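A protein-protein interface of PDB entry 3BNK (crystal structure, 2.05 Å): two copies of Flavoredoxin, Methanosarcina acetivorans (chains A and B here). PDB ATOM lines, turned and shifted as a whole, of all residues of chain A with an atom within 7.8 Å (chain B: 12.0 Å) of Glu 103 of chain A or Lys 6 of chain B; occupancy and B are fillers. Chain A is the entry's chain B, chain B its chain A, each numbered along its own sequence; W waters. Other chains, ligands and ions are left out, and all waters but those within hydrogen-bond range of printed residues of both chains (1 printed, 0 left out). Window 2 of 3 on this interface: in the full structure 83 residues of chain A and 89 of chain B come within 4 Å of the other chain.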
ATOM      1  N   PHE A 100      22.275 -11.680  14.415  1.00  0.00           N
ATOM      2  CA  PHE A 100      21.717 -10.720  15.363  1.00  0.00           C
ATOM      3  C   PHE A 100      22.835  -9.924  16.045  1.00  0.00           C
ATOM      4  O   PHE A 100      23.961 -10.404  16.209  1.00  0.00           O
ATOM      5  CB  PHE A 100      20.773 -11.404  16.380  1.00  0.00           C
ATOM      6  CG  PHE A 100      21.476 -12.167  17.483  1.00  0.00           C
ATOM      7  CD1 PHE A 100      21.572 -11.625  18.770  1.00  0.00           C
ATOM      8  CD2 PHE A 100      22.025 -13.430  17.252  1.00  0.00           C
ATOM      9  CE1 PHE A 100      22.225 -12.309  19.803  1.00  0.00           C
ATOM     10  CE2 PHE A 100      22.669 -14.127  18.281  1.00  0.00           C
ATOM     11  CZ  PHE A 100      22.769 -13.553  19.560  1.00  0.00           C
ATOM     12  N   TYR A 101      22.513  -8.690  16.410  1.00  0.00           N
ATOM     13  CA  TYR A 101      23.422  -7.822  17.128  1.00  0.00           C
ATOM     14  C   TYR A 101      22.905  -7.607  18.538  1.00  0.00           C
ATOM     15  O   TYR A 101      21.762  -7.963  18.859  1.00  0.00           O
ATOM     16  CB  TYR A 101      23.573  -6.493  16.385  1.00  0.00           C
ATOM     17  CG  TYR A 101      24.368  -6.604  15.097  1.00  0.00           C
ATOM     18  CD1 TYR A 101      23.731  -6.914  13.884  1.00  0.00           C
ATOM     19  CD2 TYR A 101      25.750  -6.414  15.089  1.00  0.00           C
ATOM     20  CE1 TYR A 101      24.459  -7.021  12.686  1.00  0.00           C
ATOM     21  CE2 TYR A 101      26.491  -6.512  13.896  1.00  0.00           C
ATOM     22  CZ  TYR A 101      25.836  -6.819  12.701  1.00  0.00           C
ATOM     23  OH  TYR A 101      26.547  -6.924  11.520  1.00  0.00           O
ATOM     24  N   GLY A 102      23.768  -7.050  19.385  1.00  0.00           N
ATOM     25  CA  GLY A 102      23.440  -6.823  20.792  1.00  0.00           C
ATOM     26  C   GLY A 102      23.823  -5.430  21.235  1.00  0.00           C
ATOM     27  O   GLY A 102      23.826  -4.500  20.424  1.00  0.00           O
ATOM     28  N   GLU A 103      24.181  -5.310  22.513  1.00  0.00           N
ATOM     29  CA  GLU A 103      24.413  -4.014  23.181  1.00  0.00           C
ATOM     30  C   GLU A 103      25.534  -3.174  22.560  1.00  0.00           C
ATOM     31  O   GLU A 103      25.480  -1.939  22.576  1.00  0.00           O
ATOM     32  CB  GLU A 103      24.685  -4.220  24.679  1.00  0.00           C
ATOM     33  CG  GLU A 103      23.504  -4.789  25.487  1.00  0.00           C
ATOM     34  CD  GLU A 103      23.871  -5.180  26.931  1.00  0.00           C
ATOM     35  OE1 GLU A 103      24.979  -4.843  27.411  1.00  0.00           O
ATOM     36  OE2 GLU A 103      23.032  -5.824  27.605  1.00  0.00           O
ATOM     37  N   LEU A 104      26.537  -3.851  22.003  1.00  0.00           N
ATOM     38  CA  LEU A 104      27.672  -3.174  21.379  1.00  0.00           C
ATOM     39  C   LEU A 104      27.364  -2.752  19.945  1.00  0.00           C
ATOM     40  O   LEU A 104      28.132  -2.010  19.348  1.00  0.00           O
ATOM     41  CB  LEU A 104      28.925  -4.052  21.422  1.00  0.00           C
ATOM     42  CG  LEU A 104      29.467  -4.453  22.795  1.00  0.00           C
ATOM     43  CD1 LEU A 104      30.721  -5.276  22.630  1.00  0.00           C
ATOM     44  CD2 LEU A 104      29.729  -3.248  23.742  1.00  0.00           C
ATOM     45  N   LYS A 105      26.248  -3.239  19.403  1.00  0.00           N
ATOM     46  CA  LYS A 105      25.687  -2.769  18.117  1.00  0.00           C
ATOM     47  C   LYS A 105      26.434  -3.268  16.875  1.00  0.00           C
ATOM     48  O   LYS A 105      25.880  -3.337  15.780  1.00  0.00           O
ATOM     49  CB  LYS A 105      25.596  -1.227  18.088  1.00  0.00           C
ATOM     50  CG  LYS A 105      25.011  -0.587  19.364  1.00  0.00           C
ATOM     51  CD  LYS A 105      23.573  -0.141  19.196  1.00  0.00           C
ATOM     52  CE  LYS A 105      22.559  -1.274  19.295  1.00  0.00           C
ATOM     53  NZ  LYS A 105      21.191  -0.877  18.734  1.00  0.00           N
ATOM     54  N   THR A 106      27.686  -3.646  17.058  1.00  0.00           N
ATOM     55  CA  THR A 106      28.604  -3.778  15.933  1.00  0.00           C
ATOM     56  C   THR A 106      29.344  -5.124  15.873  1.00  0.00           C
ATOM     57  O   THR A 106      30.184  -5.345  14.994  1.00  0.00           O
ATOM     58  CB  THR A 106      29.615  -2.628  15.985  1.00  0.00           C
ATOM     59  OG1 THR A 106      30.455  -2.684  14.837  1.00  0.00           O
ATOM     60  CG2 THR A 106      30.474  -2.745  17.196  1.00  0.00           C
ATOM     61  N   ALA A 107      29.061  -5.995  16.831  1.00  0.00           N
ATOM     62  CA  ALA A 107      29.609  -7.350  16.815  1.00  0.00           C
ATOM     63  C   ALA A 107      28.542  -8.360  16.389  1.00  0.00           C
ATOM     64  O   ALA A 107      27.656  -8.704  17.159  1.00  0.00           O
ATOM     65  CB  ALA A 107      30.216  -7.715  18.158  1.00  0.00           C
ATOM     66  N   MET A 109      26.481 -11.577  15.730  1.00  0.00           N
ATOM     67  CA  MET A 109      26.368 -12.876  16.400  1.00  0.00           C
ATOM     68  C   MET A 109      25.470 -13.819  15.611  1.00  0.00           C
ATOM     69  O   MET A 109      24.638 -13.378  14.818  1.00  0.00           O
ATOM     70  CB  MET A 109      25.866 -12.707  17.834  1.00  0.00           C
ATOM     71  CG  MET A 109      26.898 -12.093  18.752  1.00  0.00           C
ATOM     72  SD  MET A 109      26.241 -11.629  20.365  1.00  0.00           S
ATOM     73  CE  MET A 109      25.242 -10.193  19.935  1.00  0.00           C
ATOM     74  N   ASN A 116      26.656 -17.259  22.518  1.00  0.00           N
ATOM     75  CA  ASN A 116      27.313 -16.098  21.893  1.00  0.00           C
ATOM     76  C   ASN A 116      27.858 -15.135  22.940  1.00  0.00           C
ATOM     77  O   ASN A 116      27.119 -14.678  23.812  1.00  0.00           O
ATOM     78  CB  ASN A 116      26.351 -15.331  20.964  1.00  0.00           C
ATOM     79  CG  ASN A 116      25.364 -16.234  20.255  1.00  0.00           C
ATOM     80  OD1 ASN A 116      24.274 -16.506  20.770  1.00  0.00           O
ATOM     81  ND2 ASN A 116      25.722 -16.677  19.049  1.00  0.00           N
ATOM     82  N   GLU A 118      29.522 -11.527  23.382  1.00  0.00           N
ATOM     83  CA  GLU A 118      29.664 -10.236  22.727  1.00  0.00           C
ATOM     84  C   GLU A 118      30.762  -9.454  23.453  1.00  0.00           C
ATOM     85  O   GLU A 118      30.644  -9.184  24.642  1.00  0.00           O
ATOM     86  CB  GLU A 118      28.318  -9.500  22.752  1.00  0.00           C
ATOM     87  CG  GLU A 118      28.276  -8.143  22.054  1.00  0.00           C
ATOM     88  CD  GLU A 118      26.910  -7.446  22.203  1.00  0.00           C
ATOM     89  OE1 GLU A 118      26.151  -7.783  23.143  1.00  0.00           O
ATOM     90  OE2 GLU A 118      26.605  -6.561  21.371  1.00  0.00           O
ATOM     91  N   ILE A 138      30.890  -8.390  27.499  1.00  0.00           N
ATOM     92  CA  ILE A 138      29.953  -7.405  28.007  1.00  0.00           C
ATOM     93  C   ILE A 138      28.545  -7.978  28.065  1.00  0.00           C
ATOM     94  O   ILE A 138      27.769  -7.624  28.952  1.00  0.00           O
ATOM     95  CB  ILE A 138      30.018  -6.063  27.235  1.00  0.00           C
ATOM     96  CG1 ILE A 138      29.493  -6.222  25.814  1.00  0.00           C
ATOM     97  CG2 ILE A 138      31.442  -5.462  27.292  1.00  0.00           C
ATOM     98  CD1 ILE A 138      28.005  -5.820  25.647  1.00  0.00           C
ATOM     99  N   ALA A 139      28.231  -8.878  27.137  1.00  0.00           N
ATOM    100  CA  ALA A 139      26.963  -9.603  27.172  1.00  0.00           C
ATOM    101  C   ALA A 139      27.155 -11.022  26.662  1.00  0.00           C
ATOM    102  O   ALA A 139      27.968 -11.268  25.757  1.00  0.00           O
ATOM    103  CB  ALA A 139      25.877  -8.870  26.367  1.00  0.00           C
ATOM    104  N   ALA A 140      26.421 -11.941  27.278  1.00  0.00           N
ATOM    105  CA  ALA A 140      26.398 -13.337  26.882  1.00  0.00           C
ATOM    106  C   ALA A 140      24.970 -13.785  26.657  1.00  0.00           C
ATOM    107  O   ALA A 140      24.072 -13.447  27.438  1.00  0.00           O
ATOM    108  CB  ALA A 140      27.081 -14.209  27.927  1.00  0.00           C
ATOM    109  N   TYR A 141      24.774 -14.536  25.576  1.00  0.00           N
ATOM    110  CA  TYR A 141      23.459 -15.002  25.140  1.00  0.00           C
ATOM    111  C   TYR A 141      23.441 -16.516  24.959  1.00  0.00           C
ATOM    112  O   TYR A 141      24.346 -17.099  24.357  1.00  0.00           O
ATOM    113  CB  TYR A 141      23.061 -14.343  23.809  1.00  0.00           C
ATOM    114  CG  TYR A 141      23.167 -12.830  23.783  1.00  0.00           C
ATOM    115  CD1 TYR A 141      24.382 -12.199  23.519  1.00  0.00           C
ATOM    116  CD2 TYR A 141      22.042 -12.028  24.023  1.00  0.00           C
ATOM    117  CE1 TYR A 141      24.488 -10.803  23.502  1.00  0.00           C
ATOM    118  CE2 TYR A 141      22.129 -10.634  23.996  1.00  0.00           C
ATOM    119  CZ  TYR A 141      23.357 -10.031  23.740  1.00  0.00           C
ATOM    120  OH  TYR A 141      23.448  -8.658  23.716  1.00  0.00           O
ATOM    121  N   SER A 142      22.397 -17.146  25.474  1.00  0.00           N
ATOM    122  CA  SER A 142      22.080 -18.509  25.085  1.00  0.00           C
ATOM    123  C   SER A 142      20.569 -18.672  24.945  1.00  0.00           C
ATOM    124  O   SER A 142      19.850 -17.707  24.677  1.00  0.00           O
ATOM    125  CB  SER A 142      22.661 -19.518  26.081  1.00  0.00           C
ATOM    126  OG  SER A 142      22.562 -20.839  25.575  1.00  0.00           O
ATOM    127  N   GLU A 143      20.100 -19.908  25.089  1.00  0.00           N
ATOM    128  CA  GLU A 143      18.671 -20.224  25.053  1.00  0.00           C
ATOM    129  C   GLU A 143      18.395 -21.197  26.200  1.00  0.00           C
ATOM    130  O   GLU A 143      19.309 -21.883  26.676  1.00  0.00           O
ATOM    131  CB  GLU A 143      18.289 -20.846  23.708  1.00  0.00           C
ATOM    132  CG  GLU A 143      18.864 -20.119  22.501  1.00  0.00           C
ATOM    133  CD  GLU A 143      18.532 -20.780  21.192  1.00  0.00           C
ATOM    134  OE1 GLU A 143      17.592 -21.604  21.153  1.00  0.00           O
ATOM    135  OE2 GLU A 143      19.220 -20.470  20.191  1.00  0.00           O
ATOM    136  N   LEU A 147      20.635 -24.610  28.881  1.00  0.00           N
ATOM    137  CA  LEU A 147      20.982 -24.249  30.255  1.00  0.00           C
ATOM    138  C   LEU A 147      20.552 -25.287  31.279  1.00  0.00           C
ATOM    139  O   LEU A 147      19.507 -25.925  31.132  1.00  0.00           O
ATOM    140  CB  LEU A 147      20.401 -22.874  30.620  1.00  0.00           C
ATOM    141  CG  LEU A 147      20.713 -21.698  29.687  1.00  0.00           C
ATOM    142  CD1 LEU A 147      19.934 -20.472  30.132  1.00  0.00           C
ATOM    143  CD2 LEU A 147      22.197 -21.389  29.615  1.00  0.00           C
ATOM    144  N   GLY A 150      20.334 -22.178  35.048  1.00  0.00           N
ATOM    145  CA  GLY A 150      20.805 -20.862  34.574  1.00  0.00           C
ATOM    146  C   GLY A 150      22.140 -20.791  33.828  1.00  0.00           C
ATOM    147  O   GLY A 150      22.511 -19.729  33.327  1.00  0.00           O
ATOM    148  N   ALA B   2      14.179 -21.400  21.491  1.00  0.00           N
ATOM    149  CA  ALA B   2      13.434 -20.217  20.952  1.00  0.00           C
ATOM    150  C   ALA B   2      14.285 -18.937  20.950  1.00  0.00           C
ATOM    151  O   ALA B   2      15.372 -18.903  20.365  1.00  0.00           O
ATOM    152  CB  ALA B   2      12.122 -20.013  21.729  1.00  0.00           C
ATOM    153  N   GLU B   3      13.777 -17.894  21.609  1.00  0.00           N
ATOM    154  CA  GLU B   3      14.430 -16.581  21.674  1.00  0.00           C
ATOM    155  C   GLU B   3      15.747 -16.610  22.472  1.00  0.00           C
ATOM    156  O   GLU B   3      15.929 -17.454  23.359  1.00  0.00           O
ATOM    157  CB  GLU B   3      13.464 -15.546  22.284  1.00  0.00           C
ATOM    158  CG  GLU B   3      12.142 -15.372  21.518  1.00  0.00           C
ATOM    159  CD  GLU B   3      11.281 -14.216  22.043  1.00  0.00           C
ATOM    160  OE1 GLU B   3      11.852 -13.220  22.565  1.00  0.00           O
ATOM    161  OE2 GLU B   3      10.029 -14.302  21.922  1.00  0.00           O
ATOM    162  N   LYS B   4      16.659 -15.688  22.145  1.00  0.00           N
ATOM    163  CA  LYS B   4      17.918 -15.528  22.878  1.00  0.00           C
ATOM    164  C   LYS B   4      17.686 -14.904  24.251  1.00  0.00           C
ATOM    165  O   LYS B   4      16.936 -13.937  24.386  1.00  0.00           O
ATOM    166  CB  LYS B   4      18.906 -14.660  22.090  1.00  0.00           C
ATOM    167  CG  LYS B   4      19.467 -15.305  20.829  1.00  0.00           C
ATOM    168  CD  LYS B   4      20.411 -16.451  21.167  1.00  0.00           C
ATOM    169  CE  LYS B   4      20.540 -17.385  19.989  1.00  0.00           C
ATOM    170  NZ  LYS B   4      21.755 -18.218  20.064  1.00  0.00           N
ATOM    171  N   ILE B   5      18.329 -15.465  25.268  1.00  0.00           N
ATOM    172  CA  ILE B   5      18.242 -14.910  26.617  1.00  0.00           C
ATOM    173  C   ILE B   5      19.637 -14.600  27.165  1.00  0.00           C
ATOM    174  O   ILE B   5      20.571 -15.389  26.982  1.00  0.00           O
ATOM    175  CB  ILE B   5      17.451 -15.834  27.581  1.00  0.00           C
ATOM    176  CG1 ILE B   5      18.170 -17.175  27.785  1.00  0.00           C
ATOM    177  CG2 ILE B   5      16.006 -16.036  27.068  1.00  0.00           C
ATOM    178  CD1 ILE B   5      17.931 -17.797  29.154  1.00  0.00           C
ATOM    179  N   LYS B   6      19.779 -13.438  27.799  1.00  0.00           N
ATOM    180  CA  LYS B   6      21.052 -13.044  28.390  1.00  0.00           C
ATOM    181  C   LYS B   6      21.298 -13.850  29.635  1.00  0.00           C
ATOM    182  O   LYS B   6      20.387 -14.040  30.446  1.00  0.00           O
ATOM    183  CB  LYS B   6      21.094 -11.554  28.730  1.00  0.00           C
ATOM    184  CG  LYS B   6      21.606 -10.689  27.607  1.00  0.00           C
ATOM    185  CD  LYS B   6      21.469  -9.202  27.908  1.00  0.00           C
ATOM    186  CE  LYS B   6      21.606  -8.409  26.619  1.00  0.00           C
ATOM    187  NZ  LYS B   6      20.860  -7.117  26.625  1.00  0.00           N
ATOM    188  N   ILE B   7      22.527 -14.342  29.759  1.00  0.00           N
ATOM    189  CA  ILE B   7      22.993 -15.028  30.955  1.00  0.00           C
ATOM    190  C   ILE B   7      24.187 -14.260  31.520  1.00  0.00           C
ATOM    191  O   ILE B   7      24.583 -13.226  30.961  1.00  0.00           O
ATOM    192  CB  ILE B   7      23.321 -16.559  30.710  1.00  0.00           C
ATOM    193  CG1 ILE B   7      24.702 -16.771  30.055  1.00  0.00           C
ATOM    194  CG2 ILE B   7      22.158 -17.275  29.976  1.00  0.00           C
ATOM    195  CD1 ILE B   7      24.705 -16.909  28.558  1.00  0.00           C
ATOM    196  N   ASN B   8      24.747 -14.768  32.617  1.00  0.00           N
ATOM    197  CA  ASN B   8      25.827 -14.108  33.350  1.00  0.00           C
ATOM    198  C   ASN B   8      27.105 -13.973  32.514  1.00  0.00           C
ATOM    199  O   ASN B   8      27.500 -14.911  31.830  1.00  0.00           O
ATOM    200  CB  ASN B   8      26.105 -14.871  34.648  1.00  0.00           C
ATOM    201  CG  ASN B   8      26.961 -14.081  35.627  1.00  0.00           C
ATOM    202  OD1 ASN B   8      28.185 -14.011  35.486  1.00  0.00           O
ATOM    203  ND2 ASN B   8      26.314 -13.493  36.646  1.00  0.00           N
ATOM    204  N   ASN B   9      27.737 -12.799  32.597  1.00  0.00           N
ATOM    205  CA  ASN B   9      28.928 -12.445  31.811  1.00  0.00           C
ATOM    206  C   ASN B   9      30.204 -13.209  32.110  1.00  0.00           C
ATOM    207  O   ASN B   9      31.088 -13.276  31.259  1.00  0.00           O
ATOM    208  CB  ASN B   9      29.232 -10.956  31.948  1.00  0.00           C
ATOM    209  CG  ASN B   9      28.360 -10.115  31.089  1.00  0.00           C
ATOM    210  OD1 ASN B   9      28.213  -8.917  31.328  1.00  0.00           O
ATOM    211  ND2 ASN B   9      27.760 -10.728  30.075  1.00  0.00           N
ATOM    212  N   ASN B  10      30.321 -13.745  33.322  1.00  0.00           N
ATOM    213  CA  ASN B  10      31.471 -14.557  33.684  1.00  0.00           C
ATOM    214  C   ASN B  10      31.333 -15.953  33.047  1.00  0.00           C
ATOM    215  O   ASN B  10      30.999 -16.938  33.708  1.00  0.00           O
ATOM    216  CB  ASN B  10      31.614 -14.613  35.210  1.00  0.00           C
ATOM    217  CG  ASN B  10      32.934 -15.233  35.672  1.00  0.00           C
ATOM    218  OD1 ASN B  10      33.100 -15.551  36.861  1.00  0.00           O
ATOM    219  ND2 ASN B  10      33.874 -15.396  34.756  1.00  0.00           N
ATOM    220  N   VAL B  11      31.571 -16.007  31.737  1.00  0.00           N
ATOM    221  CA  VAL B  11      31.434 -17.238  30.967  1.00  0.00           C
ATOM    222  C   VAL B  11      32.793 -17.792  30.548  1.00  0.00           C
ATOM    223  O   VAL B  11      33.671 -17.048  30.077  1.00  0.00           O
ATOM    224  CB  VAL B  11      30.516 -17.045  29.738  1.00  0.00           C
ATOM    225  CG1 VAL B  11      29.060 -17.121  30.144  1.00  0.00           C
ATOM    226  CG2 VAL B  11      30.783 -15.717  29.092  1.00  0.00           C
ATOM    227  N   TYR B  14      33.752 -23.308  26.355  1.00  0.00           N
ATOM    228  CA  TYR B  14      33.138 -24.642  26.380  1.00  0.00           C
ATOM    229  C   TYR B  14      33.714 -25.588  25.329  1.00  0.00           C
ATOM    230  O   TYR B  14      33.411 -25.461  24.147  1.00  0.00           O
ATOM    231  CB  TYR B  14      31.607 -24.542  26.246  1.00  0.00           C
ATOM    232  CG  TYR B  14      30.959 -24.065  27.527  1.00  0.00           C
ATOM    233  CD1 TYR B  14      30.838 -22.703  27.796  1.00  0.00           C
ATOM    234  CD2 TYR B  14      30.480 -24.978  28.486  1.00  0.00           C
ATOM    235  CE1 TYR B  14      30.262 -22.247  28.990  1.00  0.00           C
ATOM    236  CE2 TYR B  14      29.892 -24.531  29.676  1.00  0.00           C
ATOM    237  CZ  TYR B  14      29.794 -23.159  29.914  1.00  0.00           C
ATOM    238  OH  TYR B  14      29.236 -22.680  31.080  1.00  0.00           O
HETATM  239  O   HOH W   1      25.038 -10.788  29.940  1.00  0.00           O
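The backbone NH of Ala 2 of chain B is in hydrogen-bond range of the side-chain carboxylate of Glu 143 of chain A, 3.4 Å away.
The side-chain amide oxygen (OD1) of Asn 116 of chain A sits at hydrogen-bond distance from the side-chain amino group (NZ) of Lys 4 of chain B, 3.1 Å away.
NZ of Lys 4 of chain B lies within salt-bridge range of OE2 of Glu 143 of chain A (3.4 Å).
The backbone NH (N) of Ile 5 of chain B lies within hydrogen-bond range of the backbone carbonyl oxygen (O) of Ser 142 of chain A, at 2.8 Å.
NZ of Lys 6 of chain B is in salt-bridge range of OE2 of Glu 103 of chain A, at 2.7 Å.
N of Ile 7 of chain B is in hydrogen-bond range of O of Ala 140 of chain A, at 2.9 Å.
The side-chain amide oxygen (OD1) of Asn 9 of chain B lies close to the backbone carbonyl oxygen (O) of Ile 138 of chain A, at 2.7 Å.
The side-chain amide nitrogen (ND2) of Asn 9 of chain B lies close to the backbone NH (N) of Ala 140 of chain A (3.3 Å).
The side-chain amide oxygen (OD1) of Asn 8 of chain B is in hydrogen-bond range of the backbone NH (N) of Asn 10 of chain B, 3.1 Å away.
The backbone NH (N) of Met 109 of chain A is in hydrogen-bond range of the backbone carbonyl oxygen (O) of Phe 100 of chain A, at 2.8 Å.
The backbone carbonyl oxygen of Asn 116 of chain A lies within hydrogen-bond range of the backbone NH of Tyr 141 of chain A.
The backbone NH (N) of Ile 138 of chain A lies within hydrogen-bond range of the backbone carbonyl oxygen (O) of Glu 118 of chain A (3.0 Å).
The backbone NH (N) of Glu 118 of chain A is in hydrogen-bond range of the backbone carbonyl oxygen (O) of Ala 139 of chain A (2.9 Å).
OH of Tyr 141 of chain A is in hydrogen-bond range of OE1 of Glu 118 of chain A, 2.9 Å away.
Lys 4 of chain B touches Phe 100 of chain A (CG to CZ, 3.9 Å).
Asn 9 of chain B touches Ala 139 of chain A.
Ala 140 of chain A touches Lys 6 of chain B (O to CA, 3.2 Å).
O of Asn 8 of chain B touches CB of Ala 140 of chain A (3.99 Å).
O of Ile 5 of chain B touches CA of Tyr 141 of chain A, 3.4 Å away.
Lys 6 of chain B touches Tyr 141 of chain A (CE to OH, 3.4 Å).
Tyr 141 of chain A touches Ile 7 of chain B (N to CD1, 3.8 Å).
Ser 142 of chain A touches Ile 7 of chain B.
CD1 of Leu 147 of chain A touches CD1 of Ile 5 of chain B (3.5 Å).
Leu 147 of chain A touches Ile 7 of chain B.
No residue of chain B comes within 4 Å of Gly 102 of chain A.
Printed residues of chain B within 4 Å of Glu 103 of chain A: Lys 6.
No residue of chain B comes within 4 Å of Leu 104 of chain A.
No residue of chain B comes within 4 Å of Lys 105 of chain A.
Thr 106 of chain A touches none of the printed residues of chain B.
Ala 139 of chain A touches just one residue of chain B: Asn 9.
Of chain B, only Ile 5 (3.4 Å), Lys 6 (3.4 Å) and Ile 7 (3.8 Å) come within 4 Å of Tyr 141 of chain A.
Of the printed residues of chain B, Leu 147 of chain A touches Ile 5 and Ile 7.
Of chain A, only Glu 103 (2.7 Å), Ala 140 (3.2 Å) and Tyr 141 (3.4 Å) come within 4 Å of Lys 6 of chain B.
Printed residues of chain A within 4 Å of Ile 7 of chain B: Ala 140, Tyr 141, Ser 142 and Leu 147.
Printed residues of chain A within 4 Å of Asn 9 of chain B: Ile 138, Ala 139 and Ala 140.
The nearest residue of chain A that does not touch Lys 6 of chain B is Ala 139 of chain A (4.3 Å).
The nearest printed residue of chain A that does not touch Ile 7 of chain B is Gly 150 of chain A (4.2 Å).
Printed residues of chain B that touch a printed residue of chain A: Ala 2, Lys 4, Ile 5, Lys 6, Ile 7, Asn 8 and Asn 9.
Hydrophobic or aromatic side chains of chain B that line the printed part of chain A: Ile 5 and Ile 7.
Among the printed residues, 19 pairs touch across the chains.
Among the printed residues, Asp or Glu carboxylates within 4 Å of a Lys or Arg side-chain nitrogen of the other chain: Glu 103 of chain A with Lys 6 of chain B and Glu 143 of chain A with Lys 4 of chain B.
No position is printed for both chains.
Of the 19 pairs that touch across the chains among the printed residues, none has its exchanged pair printed and touching as well.
Water W1 lies within hydrogen-bond range of the backbone carbonyl oxygen (O) of Ile 7 of chain B (2.7 Å), the side-chain amide nitrogen (ND2) of Asn 9 of chain B (2.7 Å) and the backbone NH (N) of Ala 140 of chain A (3.2 Å).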
